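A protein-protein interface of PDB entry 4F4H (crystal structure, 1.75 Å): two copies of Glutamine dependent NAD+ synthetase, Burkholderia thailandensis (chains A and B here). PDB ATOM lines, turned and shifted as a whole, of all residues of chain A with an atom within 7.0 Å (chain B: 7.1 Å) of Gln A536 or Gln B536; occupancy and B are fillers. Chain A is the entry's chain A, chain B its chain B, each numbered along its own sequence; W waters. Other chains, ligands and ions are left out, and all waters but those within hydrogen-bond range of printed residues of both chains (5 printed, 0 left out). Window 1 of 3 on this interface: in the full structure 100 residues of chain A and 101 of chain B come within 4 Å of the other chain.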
ATOM      1  N   LEU A 426      28.328   6.697  31.486  1.00  0.00           N
ATOM      2  CA  LEU A 426      26.882   6.910  31.494  1.00  0.00           C
ATOM      3  C   LEU A 426      26.320   6.508  32.848  1.00  0.00           C
ATOM      4  O   LEU A 426      26.651   5.465  33.340  1.00  0.00           O
ATOM      5  CB  LEU A 426      26.182   6.068  30.398  1.00  0.00           C
ATOM      6  CG  LEU A 426      26.118   6.572  28.958  1.00  0.00           C
ATOM      7  CD1 LEU A 426      25.400   5.562  28.060  1.00  0.00           C
ATOM      8  CD2 LEU A 426      25.435   7.921  28.907  1.00  0.00           C
ATOM      9  N   TYR A 427      25.485   7.367  33.435  1.00  0.00           N
ATOM     10  CA  TYR A 427      24.726   7.039  34.701  1.00  0.00           C
ATOM     11  C   TYR A 427      25.638   6.955  35.912  1.00  0.00           C
ATOM     12  O   TYR A 427      25.188   6.607  37.006  1.00  0.00           O
ATOM     13  CB  TYR A 427      23.918   5.705  34.541  1.00  0.00           C
ATOM     14  CG  TYR A 427      23.372   5.509  33.116  1.00  0.00           C
ATOM     15  CD1 TYR A 427      22.834   6.593  32.400  1.00  0.00           C
ATOM     16  CD2 TYR A 427      23.408   4.250  32.495  1.00  0.00           C
ATOM     17  CE1 TYR A 427      22.356   6.439  31.099  1.00  0.00           C
ATOM     18  CE2 TYR A 427      22.940   4.084  31.189  1.00  0.00           C
ATOM     19  CZ  TYR A 427      22.414   5.169  30.499  1.00  0.00           C
ATOM     20  OH  TYR A 427      21.940   4.999  29.223  1.00  0.00           O
ATOM     21  N   MET A 430      28.537  10.804  35.063  1.00  0.00           N
ATOM     22  CA  MET A 430      27.656  11.674  34.256  1.00  0.00           C
ATOM     23  C   MET A 430      26.261  11.823  34.843  1.00  0.00           C
ATOM     24  O   MET A 430      25.450  12.530  34.271  1.00  0.00           O
ATOM     25  CB  MET A 430      27.517  11.136  32.817  1.00  0.00           C
ATOM     26  CG  MET A 430      28.833  11.024  32.072  1.00  0.00           C
ATOM     27  SD  MET A 430      28.651  10.239  30.443  1.00  0.00           S
ATOM     28  CE  MET A 430      27.532  11.415  29.634  1.00  0.00           C
ATOM     29  N   ALA A 431      25.987  11.141  35.975  1.00  0.00           N
ATOM     30  CA  ALA A 431      24.662  11.209  36.628  1.00  0.00           C
ATOM     31  C   ALA A 431      24.466  12.545  37.318  1.00  0.00           C
ATOM     32  O   ALA A 431      25.137  12.867  38.291  1.00  0.00           O
ATOM     33  CB  ALA A 431      24.458  10.077  37.634  1.00  0.00           C
ATOM     34  N   GLY A 432      23.505  13.294  36.847  1.00  0.00           N
ATOM     35  CA  GLY A 432      23.122  14.532  37.508  1.00  0.00           C
ATOM     36  C   GLY A 432      22.348  15.459  36.608  1.00  0.00           C
ATOM     37  O   GLY A 432      21.925  15.090  35.518  1.00  0.00           O
ATOM     38  N   GLY A 433      22.144  16.659  37.105  1.00  0.00           N
ATOM     39  CA  GLY A 433      21.264  17.594  36.479  1.00  0.00           C
ATOM     40  C   GLY A 433      21.931  18.627  35.614  1.00  0.00           C
ATOM     41  O   GLY A 433      21.274  19.190  34.751  1.00  0.00           O
ATOM     42  N   PHE A 434      23.197  18.958  35.888  1.00  0.00           N
ATOM     43  CA  PHE A 434      23.850  20.110  35.197  1.00  0.00           C
ATOM     44  C   PHE A 434      25.350  19.902  35.191  1.00  0.00           C
ATOM     45  O   PHE A 434      25.952  19.708  36.238  1.00  0.00           O
ATOM     46  CB  PHE A 434      23.477  21.406  35.927  1.00  0.00           C
ATOM     47  CG  PHE A 434      23.712  22.670  35.140  1.00  0.00           C
ATOM     48  CD1 PHE A 434      23.116  22.871  33.897  1.00  0.00           C
ATOM     49  CD2 PHE A 434      24.433  23.712  35.687  1.00  0.00           C
ATOM     50  CE1 PHE A 434      23.303  24.071  33.193  1.00  0.00           C
ATOM     51  CE2 PHE A 434      24.585  24.927  35.003  1.00  0.00           C
ATOM     52  CZ  PHE A 434      24.048  25.088  33.749  1.00  0.00           C
ATOM     53  N   LYS A 438      31.408  21.029  31.395  1.00  0.00           N
ATOM     54  CA  LYS A 438      31.345  20.202  30.204  1.00  0.00           C
ATOM     55  C   LYS A 438      32.047  20.852  29.000  1.00  0.00           C
ATOM     56  O   LYS A 438      32.434  20.157  28.033  1.00  0.00           O
ATOM     57  CB  LYS A 438      29.840  20.012  29.853  1.00  0.00           C
ATOM     58  CG  LYS A 438      29.470  19.057  28.774  1.00  0.00           C
ATOM     59  CD  LYS A 438      27.973  19.293  28.472  1.00  0.00           C
ATOM     60  CE  LYS A 438      27.493  18.450  27.359  1.00  0.00           C
ATOM     61  NZ  LYS A 438      26.023  18.484  27.257  1.00  0.00           N
ATOM     62  N   GLU A 531      10.843  17.768  31.112  1.00  0.00           N
ATOM     63  CA  GLU A 531      11.749  18.032  30.008  1.00  0.00           C
ATOM     64  C   GLU A 531      13.186  17.636  30.349  1.00  0.00           C
ATOM     65  O   GLU A 531      13.884  17.058  29.530  1.00  0.00           O
ATOM     66  CB  GLU A 531      11.699  19.521  29.628  1.00  0.00           C
ATOM     67  CG  GLU A 531      12.450  19.878  28.370  1.00  0.00           C
ATOM     68  CD  GLU A 531      11.857  19.239  27.152  1.00  0.00           C
ATOM     69  OE1 GLU A 531      10.606  19.189  27.032  1.00  0.00           O
ATOM     70  OE2 GLU A 531      12.655  18.855  26.288  1.00  0.00           O
ATOM     71  N   TYR A 532      13.634  17.956  31.576  1.00  0.00           N
ATOM     72  CA  TYR A 532      15.011  17.713  31.984  1.00  0.00           C
ATOM     73  C   TYR A 532      15.360  16.231  31.841  1.00  0.00           C
ATOM     74  O   TYR A 532      16.478  15.874  31.484  1.00  0.00           O
ATOM     75  CB  TYR A 532      15.226  18.175  33.478  1.00  0.00           C
ATOM     76  CG  TYR A 532      14.665  17.202  34.475  1.00  0.00           C
ATOM     77  CD1 TYR A 532      13.329  17.248  34.845  1.00  0.00           C
ATOM     78  CD2 TYR A 532      15.461  16.172  35.010  1.00  0.00           C
ATOM     79  CE1 TYR A 532      12.782  16.319  35.731  1.00  0.00           C
ATOM     80  CE2 TYR A 532      14.919  15.213  35.884  1.00  0.00           C
ATOM     81  CZ  TYR A 532      13.596  15.303  36.255  1.00  0.00           C
ATOM     82  OH  TYR A 532      13.020  14.378  37.090  1.00  0.00           O
ATOM     83  N   LYS A 533      14.370  15.396  32.114  1.00  0.00           N
ATOM     84  CA  LYS A 533      14.525  13.948  32.135  1.00  0.00           C
ATOM     85  C   LYS A 533      14.554  13.366  30.714  1.00  0.00           C
ATOM     86  O   LYS A 533      15.403  12.552  30.386  1.00  0.00           O
ATOM     87  CB  LYS A 533      13.387  13.378  32.982  1.00  0.00           C
ATOM     88  CG  LYS A 533      13.337  11.890  33.068  1.00  0.00           C
ATOM     89  CD  LYS A 533      12.903  11.393  34.465  1.00  0.00           C
ATOM     90  CE  LYS A 533      11.517  11.802  34.857  1.00  0.00           C
ATOM     91  NZ  LYS A 533      11.117  11.182  36.170  1.00  0.00           N
ATOM     92  N   ARG A 534      13.631  13.785  29.875  1.00  0.00           N
ATOM     93  CA  ARG A 534      13.629  13.362  28.483  1.00  0.00           C
ATOM     94  C   ARG A 534      14.925  13.713  27.775  1.00  0.00           C
ATOM     95  O   ARG A 534      15.405  12.958  26.921  1.00  0.00           O
ATOM     96  CB  ARG A 534      12.462  13.981  27.735  1.00  0.00           C
ATOM     97  CG  ARG A 534      11.124  13.426  28.156  1.00  0.00           C
ATOM     98  CD  ARG A 534      10.028  13.912  27.264  1.00  0.00           C
ATOM     99  NE  ARG A 534       9.836  15.358  27.344  1.00  0.00           N
ATOM    100  CZ  ARG A 534       8.975  15.975  28.147  1.00  0.00           C
ATOM    101  NH1 ARG A 534       8.230  15.305  28.994  1.00  0.00           N
ATOM    102  NH2 ARG A 534       8.876  17.291  28.098  1.00  0.00           N
ATOM    103  N   ARG A 535      15.484  14.870  28.113  1.00  0.00           N
ATOM    104  CA  ARG A 535      16.674  15.389  27.408  1.00  0.00           C
ATOM    105  C   ARG A 535      17.918  14.552  27.685  1.00  0.00           C
ATOM    106  O   ARG A 535      18.935  14.757  27.032  1.00  0.00           O
ATOM    107  CB  ARG A 535      16.959  16.860  27.788  1.00  0.00           C
ATOM    108  CG  ARG A 535      15.858  17.879  27.482  1.00  0.00           C
ATOM    109  CD  ARG A 535      16.078  18.796  26.293  1.00  0.00           C
ATOM    110  NE  ARG A 535      17.412  19.386  26.289  1.00  0.00           N
ATOM    111  CZ  ARG A 535      17.706  20.679  26.335  1.00  0.00           C
ATOM    112  NH1 ARG A 535      16.772  21.643  26.352  1.00  0.00           N
ATOM    113  NH2 ARG A 535      18.973  21.014  26.360  1.00  0.00           N
ATOM    114  N   GLN A 536      17.857  13.609  28.629  1.00  0.00           N
ATOM    115  CA  GLN A 536      18.955  12.649  28.826  1.00  0.00           C
ATOM    116  C   GLN A 536      18.605  11.236  28.363  1.00  0.00           C
ATOM    117  O   GLN A 536      19.378  10.291  28.571  1.00  0.00           O
ATOM    118  CB  GLN A 536      19.371  12.607  30.297  1.00  0.00           C
ATOM    119  CG  GLN A 536      20.112  13.878  30.754  1.00  0.00           C
ATOM    120  CD  GLN A 536      20.628  13.778  32.193  1.00  0.00           C
ATOM    121  OE1 GLN A 536      21.215  12.780  32.578  1.00  0.00           O
ATOM    122  NE2 GLN A 536      20.396  14.824  32.987  1.00  0.00           N
ATOM    123  N   ALA A 537      17.447  11.074  27.765  1.00  0.00           N
ATOM    124  CA  ALA A 537      17.022   9.712  27.324  1.00  0.00           C
ATOM    125  C   ALA A 537      17.825   9.246  26.096  1.00  0.00           C
ATOM    126  O   ALA A 537      18.277  10.061  25.315  1.00  0.00           O
ATOM    127  CB  ALA A 537      15.540   9.703  26.965  1.00  0.00           C
ATOM    128  N   PRO A 538      17.932   7.922  25.894  1.00  0.00           N
ATOM    129  CA  PRO A 538      18.527   7.468  24.638  1.00  0.00           C
ATOM    130  C   PRO A 538      17.662   7.815  23.454  1.00  0.00           C
ATOM    131  O   PRO A 538      16.472   8.014  23.600  1.00  0.00           O
ATOM    132  CB  PRO A 538      18.603   5.947  24.779  1.00  0.00           C
ATOM    133  CG  PRO A 538      18.154   5.621  26.154  1.00  0.00           C
ATOM    134  CD  PRO A 538      17.479   6.821  26.743  1.00  0.00           C
ATOM    135  N   VAL A 539      18.288   7.894  22.302  1.00  0.00           N
ATOM    136  CA  VAL A 539      17.605   8.070  21.055  1.00  0.00           C
ATOM    137  C   VAL A 539      16.578   6.937  20.889  1.00  0.00           C
ATOM    138  O   VAL A 539      16.800   5.797  21.319  1.00  0.00           O
ATOM    139  CB  VAL A 539      18.628   8.089  19.878  1.00  0.00           C
ATOM    140  CG1 VAL A 539      19.359   6.776  19.764  1.00  0.00           C
ATOM    141  CG2 VAL A 539      17.928   8.415  18.570  1.00  0.00           C
ATOM    142  N   ILE A 556      14.771  23.570  28.933  1.00  0.00           N
ATOM    143  CA  ILE A 556      14.547  23.044  30.274  1.00  0.00           C
ATOM    144  C   ILE A 556      14.155  24.197  31.212  1.00  0.00           C
ATOM    145  O   ILE A 556      13.118  24.152  31.882  1.00  0.00           O
ATOM    146  CB  ILE A 556      15.796  22.301  30.818  1.00  0.00           C
ATOM    147  CG1 ILE A 556      16.085  21.082  29.950  1.00  0.00           C
ATOM    148  CG2 ILE A 556      15.593  21.936  32.284  1.00  0.00           C
ATOM    149  CD1 ILE A 556      17.474  20.476  30.158  1.00  0.00           C
ATOM    150  N   LEU B 426      15.389   8.498  35.347  1.00  0.00           N
ATOM    151  CA  LEU B 426      16.711   8.696  34.808  1.00  0.00           C
ATOM    152  C   LEU B 426      17.632   7.595  35.344  1.00  0.00           C
ATOM    153  O   LEU B 426      17.618   7.303  36.554  1.00  0.00           O
ATOM    154  CB  LEU B 426      17.303  10.072  35.234  1.00  0.00           C
ATOM    155  CG  LEU B 426      16.937  11.303  34.394  1.00  0.00           C
ATOM    156  CD1 LEU B 426      17.557  12.571  34.982  1.00  0.00           C
ATOM    157  CD2 LEU B 426      17.422  11.050  32.975  1.00  0.00           C
ATOM    158  N   TYR B 427      18.428   7.001  34.450  1.00  0.00           N
ATOM    159  CA  TYR B 427      19.468   6.022  34.835  1.00  0.00           C
ATOM    160  C   TYR B 427      18.894   4.707  35.341  1.00  0.00           C
ATOM    161  O   TYR B 427      19.642   3.835  35.792  1.00  0.00           O
ATOM    162  CB  TYR B 427      20.393   6.617  35.895  1.00  0.00           C
ATOM    163  CG  TYR B 427      20.656   8.103  35.664  1.00  0.00           C
ATOM    164  CD1 TYR B 427      20.878   8.598  34.398  1.00  0.00           C
ATOM    165  CD2 TYR B 427      20.686   8.995  36.732  1.00  0.00           C
ATOM    166  CE1 TYR B 427      21.129   9.968  34.186  1.00  0.00           C
ATOM    167  CE2 TYR B 427      20.939  10.342  36.534  1.00  0.00           C
ATOM    168  CZ  TYR B 427      21.136  10.831  35.270  1.00  0.00           C
ATOM    169  OH  TYR B 427      21.380  12.176  35.107  1.00  0.00           O
ATOM    170  N   MET B 430      15.290   4.067  32.177  1.00  0.00           N
ATOM    171  CA  MET B 430      15.787   4.801  31.001  1.00  0.00           C
ATOM    172  C   MET B 430      17.217   4.429  30.605  1.00  0.00           C
ATOM    173  O   MET B 430      17.737   4.938  29.601  1.00  0.00           O
ATOM    174  CB  MET B 430      15.719   6.299  31.274  1.00  0.00           C
ATOM    175  CG  MET B 430      14.303   6.811  31.493  1.00  0.00           C
ATOM    176  SD  MET B 430      14.281   8.556  31.880  1.00  0.00           S
ATOM    177  CE  MET B 430      14.619   9.265  30.257  1.00  0.00           C
ATOM    178  N   ALA B 431      17.883   3.579  31.400  1.00  0.00           N
ATOM    179  CA  ALA B 431      19.289   3.222  31.144  1.00  0.00           C
ATOM    180  C   ALA B 431      19.411   2.281  29.954  1.00  0.00           C
ATOM    181  O   ALA B 431      18.837   1.149  29.952  1.00  0.00           O
ATOM    182  CB  ALA B 431      19.913   2.545  32.366  1.00  0.00           C
ATOM    183  N   GLY B 432      20.151   2.706  28.950  1.00  0.00           N
ATOM    184  CA  GLY B 432      20.372   1.853  27.776  1.00  0.00           C
ATOM    185  C   GLY B 432      20.783   2.619  26.541  1.00  0.00           C
ATOM    186  O   GLY B 432      21.035   3.830  26.606  1.00  0.00           O
ATOM    187  N   GLY B 433      20.845   1.895  25.417  1.00  0.00           N
ATOM    188  CA  GLY B 433      21.372   2.428  24.215  1.00  0.00           C
ATOM    189  C   GLY B 433      20.357   2.899  23.232  1.00  0.00           C
ATOM    190  O   GLY B 433      20.687   3.708  22.345  1.00  0.00           O
ATOM    191  N   PHE B 434      19.130   2.344  23.289  1.00  0.00           N
ATOM    192  CA  PHE B 434      18.159   2.617  22.223  1.00  0.00           C
ATOM    193  C   PHE B 434      16.738   2.398  22.727  1.00  0.00           C
ATOM    194  O   PHE B 434      16.429   1.327  23.224  1.00  0.00           O
ATOM    195  CB  PHE B 434      18.484   1.693  21.003  1.00  0.00           C
ATOM    196  CG  PHE B 434      17.813   2.107  19.692  1.00  0.00           C
ATOM    197  CD1 PHE B 434      18.036   3.353  19.148  1.00  0.00           C
ATOM    198  CD2 PHE B 434      17.046   1.189  18.958  1.00  0.00           C
ATOM    199  CE1 PHE B 434      17.480   3.713  17.923  1.00  0.00           C
ATOM    200  CE2 PHE B 434      16.495   1.546  17.731  1.00  0.00           C
ATOM    201  CZ  PHE B 434      16.709   2.815  17.221  1.00  0.00           C
ATOM    202  N   LYS B 438       9.908   4.689  22.438  1.00  0.00           N
ATOM    203  CA  LYS B 438       9.827   6.038  22.949  1.00  0.00           C
ATOM    204  C   LYS B 438       8.729   6.900  22.261  1.00  0.00           C
ATOM    205  O   LYS B 438       8.282   7.904  22.844  1.00  0.00           O
ATOM    206  CB  LYS B 438      11.205   6.685  22.752  1.00  0.00           C
ATOM    207  CG  LYS B 438      11.501   8.008  23.418  1.00  0.00           C
ATOM    208  CD  LYS B 438      12.810   8.494  22.754  1.00  0.00           C
ATOM    209  CE  LYS B 438      13.245   9.844  23.224  1.00  0.00           C
ATOM    210  NZ  LYS B 438      14.572  10.233  22.708  1.00  0.00           N
ATOM    211  N   GLU B 531      30.219   9.516  20.675  1.00  0.00           N
ATOM    212  CA  GLU B 531      29.020  10.302  20.410  1.00  0.00           C
ATOM    213  C   GLU B 531      27.800   9.797  21.183  1.00  0.00           C
ATOM    214  O   GLU B 531      27.003  10.585  21.746  1.00  0.00           O
ATOM    215  CB  GLU B 531      28.731  10.341  18.918  1.00  0.00           C
ATOM    216  CG  GLU B 531      27.630  11.290  18.547  1.00  0.00           C
ATOM    217  CD  GLU B 531      27.988  12.755  18.809  1.00  0.00           C
ATOM    218  OE1 GLU B 531      29.161  13.141  18.571  1.00  0.00           O
ATOM    219  OE2 GLU B 531      27.051  13.524  19.174  1.00  0.00           O
ATOM    220  N   TYR B 532      27.646   8.480  21.227  1.00  0.00           N
ATOM    221  CA  TYR B 532      26.474   7.883  21.907  1.00  0.00           C
ATOM    222  C   TYR B 532      26.365   8.302  23.373  1.00  0.00           C
ATOM    223  O   TYR B 532      25.265   8.476  23.921  1.00  0.00           O
ATOM    224  CB  TYR B 532      26.522   6.340  21.779  1.00  0.00           C
ATOM    225  CG  TYR B 532      27.461   5.704  22.772  1.00  0.00           C
ATOM    226  CD1 TYR B 532      28.816   5.626  22.525  1.00  0.00           C
ATOM    227  CD2 TYR B 532      26.991   5.256  24.002  1.00  0.00           C
ATOM    228  CE1 TYR B 532      29.695   5.065  23.462  1.00  0.00           C
ATOM    229  CE2 TYR B 532      27.853   4.714  24.949  1.00  0.00           C
ATOM    230  CZ  TYR B 532      29.209   4.612  24.667  1.00  0.00           C
ATOM    231  OH  TYR B 532      30.083   4.075  25.599  1.00  0.00           O
ATOM    232  N   LYS B 533      27.515   8.501  23.996  1.00  0.00           N
ATOM    233  CA  LYS B 533      27.595   8.803  25.407  1.00  0.00           C
ATOM    234  C   LYS B 533      27.299  10.268  25.658  1.00  0.00           C
ATOM    235  O   LYS B 533      26.506  10.629  26.558  1.00  0.00           O
ATOM    236  CB  LYS B 533      29.018   8.402  25.891  1.00  0.00           C
ATOM    237  CG  LYS B 533      29.232   8.501  27.379  1.00  0.00           C
ATOM    238  CD  LYS B 533      30.601   7.976  27.837  1.00  0.00           C
ATOM    239  CE  LYS B 533      30.958   6.597  27.405  1.00  0.00           C
ATOM    240  NZ  LYS B 533      32.156   6.074  28.107  1.00  0.00           N
ATOM    241  N   ARG B 534      27.924  11.140  24.867  1.00  0.00           N
ATOM    242  CA  ARG B 534      27.681  12.567  24.977  1.00  0.00           C
ATOM    243  C   ARG B 534      26.216  12.928  24.760  1.00  0.00           C
ATOM    244  O   ARG B 534      25.714  13.863  25.373  1.00  0.00           O
ATOM    245  CB  ARG B 534      28.516  13.352  23.978  1.00  0.00           C
ATOM    246  CG  ARG B 534      29.988  13.429  24.378  1.00  0.00           C
ATOM    247  CD  ARG B 534      30.746  14.338  23.474  1.00  0.00           C
ATOM    248  NE  ARG B 534      30.695  13.919  22.057  1.00  0.00           N
ATOM    249  CZ  ARG B 534      31.587  13.152  21.430  1.00  0.00           C
ATOM    250  NH1 ARG B 534      32.655  12.697  22.050  1.00  0.00           N
ATOM    251  NH2 ARG B 534      31.406  12.872  20.144  1.00  0.00           N
ATOM    252  N   ARG B 535      25.542  12.195  23.876  1.00  0.00           N
ATOM    253  CA  ARG B 535      24.148  12.486  23.541  1.00  0.00           C
ATOM    254  C   ARG B 535      23.155  12.213  24.695  1.00  0.00           C
ATOM    255  O   ARG B 535      21.978  12.638  24.616  1.00  0.00           O
ATOM    256  CB  ARG B 535      23.750  11.719  22.284  1.00  0.00           C
ATOM    257  CG  ARG B 535      24.443  12.250  21.022  1.00  0.00           C
ATOM    258  CD  ARG B 535      23.609  13.104  20.086  1.00  0.00           C
ATOM    259  NE  ARG B 535      22.255  12.610  19.835  1.00  0.00           N
ATOM    260  CZ  ARG B 535      21.783  12.137  18.669  1.00  0.00           C
ATOM    261  NH1 ARG B 535      22.530  12.044  17.568  1.00  0.00           N
ATOM    262  NH2 ARG B 535      20.522  11.763  18.605  1.00  0.00           N
ATOM    263  N   GLN B 536      23.601  11.551  25.766  1.00  0.00           N
ATOM    264  CA  GLN B 536      22.790  11.411  26.972  1.00  0.00           C
ATOM    265  C   GLN B 536      23.296  12.253  28.166  1.00  0.00           C
ATOM    266  O   GLN B 536      22.774  12.135  29.270  1.00  0.00           O
ATOM    267  CB  GLN B 536      22.699   9.920  27.366  1.00  0.00           C
ATOM    268  CG  GLN B 536      21.877   9.084  26.389  1.00  0.00           C
ATOM    269  CD  GLN B 536      21.728   7.628  26.862  1.00  0.00           C
ATOM    270  OE1 GLN B 536      21.368   7.367  28.025  1.00  0.00           O
ATOM    271  NE2 GLN B 536      22.043   6.679  25.977  1.00  0.00           N
ATOM    272  N   ALA B 537      24.286  13.112  27.932  1.00  0.00           N
ATOM    273  CA  ALA B 537      24.864  13.921  28.984  1.00  0.00           C
ATOM    274  C   ALA B 537      23.871  15.007  29.436  1.00  0.00           C
ATOM    275  O   ALA B 537      23.064  15.469  28.651  1.00  0.00           O
ATOM    276  CB  ALA B 537      26.176  14.577  28.500  1.00  0.00           C
ATOM    277  N   PRO B 538      23.954  15.436  30.712  1.00  0.00           N
ATOM    278  CA  PRO B 538      23.212  16.612  31.118  1.00  0.00           C
ATOM    279  C   PRO B 538      23.680  17.830  30.327  1.00  0.00           C
ATOM    280  O   PRO B 538      24.802  17.856  29.805  1.00  0.00           O
ATOM    281  CB  PRO B 538      23.591  16.790  32.612  1.00  0.00           C
ATOM    282  CG  PRO B 538      24.226  15.492  32.999  1.00  0.00           C
ATOM    283  CD  PRO B 538      24.837  14.935  31.776  1.00  0.00           C
ATOM    284  N   VAL B 539      22.810  18.827  30.236  1.00  0.00           N
ATOM    285  CA  VAL B 539      23.169  20.115  29.680  1.00  0.00           C
ATOM    286  C   VAL B 539      24.311  20.696  30.479  1.00  0.00           C
ATOM    287  O   VAL B 539      24.424  20.458  31.683  1.00  0.00           O
ATOM    288  CB  VAL B 539      21.949  21.101  29.714  1.00  0.00           C
ATOM    289  CG1 VAL B 539      21.369  21.212  31.076  1.00  0.00           C
ATOM    290  CG2 VAL B 539      22.349  22.483  29.193  1.00  0.00           C
ATOM    291  N   ILE B 556      24.768   9.466  15.643  1.00  0.00           N
ATOM    292  CA  ILE B 556      25.424   8.329  16.345  1.00  0.00           C
ATOM    293  C   ILE B 556      25.806   7.250  15.331  1.00  0.00           C
ATOM    294  O   ILE B 556      26.968   6.777  15.279  1.00  0.00           O
ATOM    295  CB  ILE B 556      24.522   7.718  17.441  1.00  0.00           C
ATOM    296  CG1 ILE B 556      24.236   8.783  18.507  1.00  0.00           C
ATOM    297  CG2 ILE B 556      25.174   6.437  17.994  1.00  0.00           C
ATOM    298  CD1 ILE B 556      23.174   8.396  19.557  1.00  0.00           C
HETATM  299  O   HOH W   1      26.547  16.429  25.269  1.00  0.00           O
HETATM  300  O   HOH W   2      14.199  12.272  24.385  1.00  0.00           O
HETATM  301  O   HOH W   3      20.687  16.581  28.121  1.00  0.00           O
HETATM  302  O   HOH W   4      20.139  10.698  23.400  1.00  0.00           O
HETATM  303  O   HOH W   5      22.117  10.135  31.268  1.00  0.00           O
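The side-chain hydroxyl of Tyr A427 is in hydrogen-bond range of the backbone NH of Gly B432 (2.9 Å).
The side-chain hydroxyl of Tyr A427 lies within hydrogen-bond range of the side-chain amide oxygen of Gln B536 (2.7 Å).
OH of Tyr B427 sits at hydrogen-bond distance from N of Gly A432.
The side-chain amino group of Lys A438 lies within hydrogen-bond range of the backbone carbonyl oxygen of Pro B538, 2.9 Å away.
OE1 of Gln A536 lies within hydrogen-bond range of OH of Tyr B427 (2.6 Å).
NZ of Lys B438 sits at hydrogen-bond distance from O of Pro A538 (3.1 Å).
N of Leu A426 is in hydrogen-bond range of SD of Met A430, 3.7 Å away.
NE2 of Gln A536 sits at hydrogen-bond distance from O of Gly A432 (3.0 Å).
The backbone NH (N) of Leu B426 sits at hydrogen-bond distance from the side-chain sulfur (SD) of Met B430 (3.6 Å).
O of Gly B432 is in hydrogen-bond range of NE2 of Gln B536 (3.1 Å).
Among the printed residues, merely in contact across the chains: Met A430 with Lys B533, Lys A533 with Met B430, Pro A538 with Gly B432, Pro A538 with Met B430, Gly A432 with Pro B538, Tyr A427 with Tyr B427, Ala A537 with Met B430, Met A430 with Pro B538, Val A539 with Phe B434, Gln A536 with Gln B536, Phe A434 with Val B539, Tyr A427 with Ala B431, Lys A533 with Leu B426, Met A430 with Ala B537, Gln A536 with Leu B426, Ala A431 with Tyr B427, Pro A538 with Gln B536, Leu A426 with Gln B536, Leu A426 with Lys B533, Gln A536 with Pro B538, Tyr A532 with Leu B426, Pro A538 with Gly B433, Ala A537 with Gln B536, Gly A433 with Pro B538, Pro A538 with Phe B434, Phe A434 with Pro B538 and Gln A536 with Ala B537.
Of the printed residues of chain B, Gly A433 touches Pro B538.
Printed residues of chain B within 4 Å of Lys A533: Leu B426 and Met B430.
Arg A535 touches none of the printed residues of chain B.
Gln A536 touches just these residues of chain B: Leu B426, Tyr B427, Gln B536, Ala B537 and Pro B538.
Arg B535 touches none of the printed residues of chain A.
Gln B536 touches just these residues of chain A: Leu A426, Tyr A427, Gln A536, Ala A537 and Pro A538.
Of the printed residues of chain A, Val B539 touches Phe A434.
Printed residues of chain A that touch a printed residue of chain B: Leu A426, Tyr A427, Met A430, Ala A431, Gly A432, Gly A433, Phe A434, Lys A438, Tyr A532, Lys A533, Gln A536, Ala A537, Pro A538 and Val A539.
Of the 18 printed residues of chain B, 13 touch a printed residue of chain A.
Hydrophobic or aromatic side chains of chain B that line the printed part of chain A: Leu B426, Tyr B427, Met B430, Ala B431, Phe B434, Ala B537, Pro B538 and Val B539.
Among the printed residues, 33 pairs touch across the chains.
Among the printed residues, no Asp or Glu carboxylate lies within 4 Å of a Lys or Arg side-chain nitrogen of the other chain.
Leu A426 touches Lys B533, and with the chains exchanged Lys A533 touches Leu B426.
Tyr A427 touches Gln B536, and with the chains exchanged Gln A536 touches Tyr B427.
Met A430 touches Pro B538, and with the chains exchanged Pro A538 touches Met B430.
Lys A438 touches Pro B538, and with the chains exchanged Pro A538 touches Lys B438.
18 positions are printed for both chains.
Water W3 bridges the backbone carbonyl oxygen (O) of Ala B537 and the backbone carbonyl oxygen (O) of Arg A535.
Water W1 lies within hydrogen-bond range of O of Arg B534 and NZ of Lys A438.
Water W4 lies within hydrogen-bond range of O of Ala A537 and O of Arg B535.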
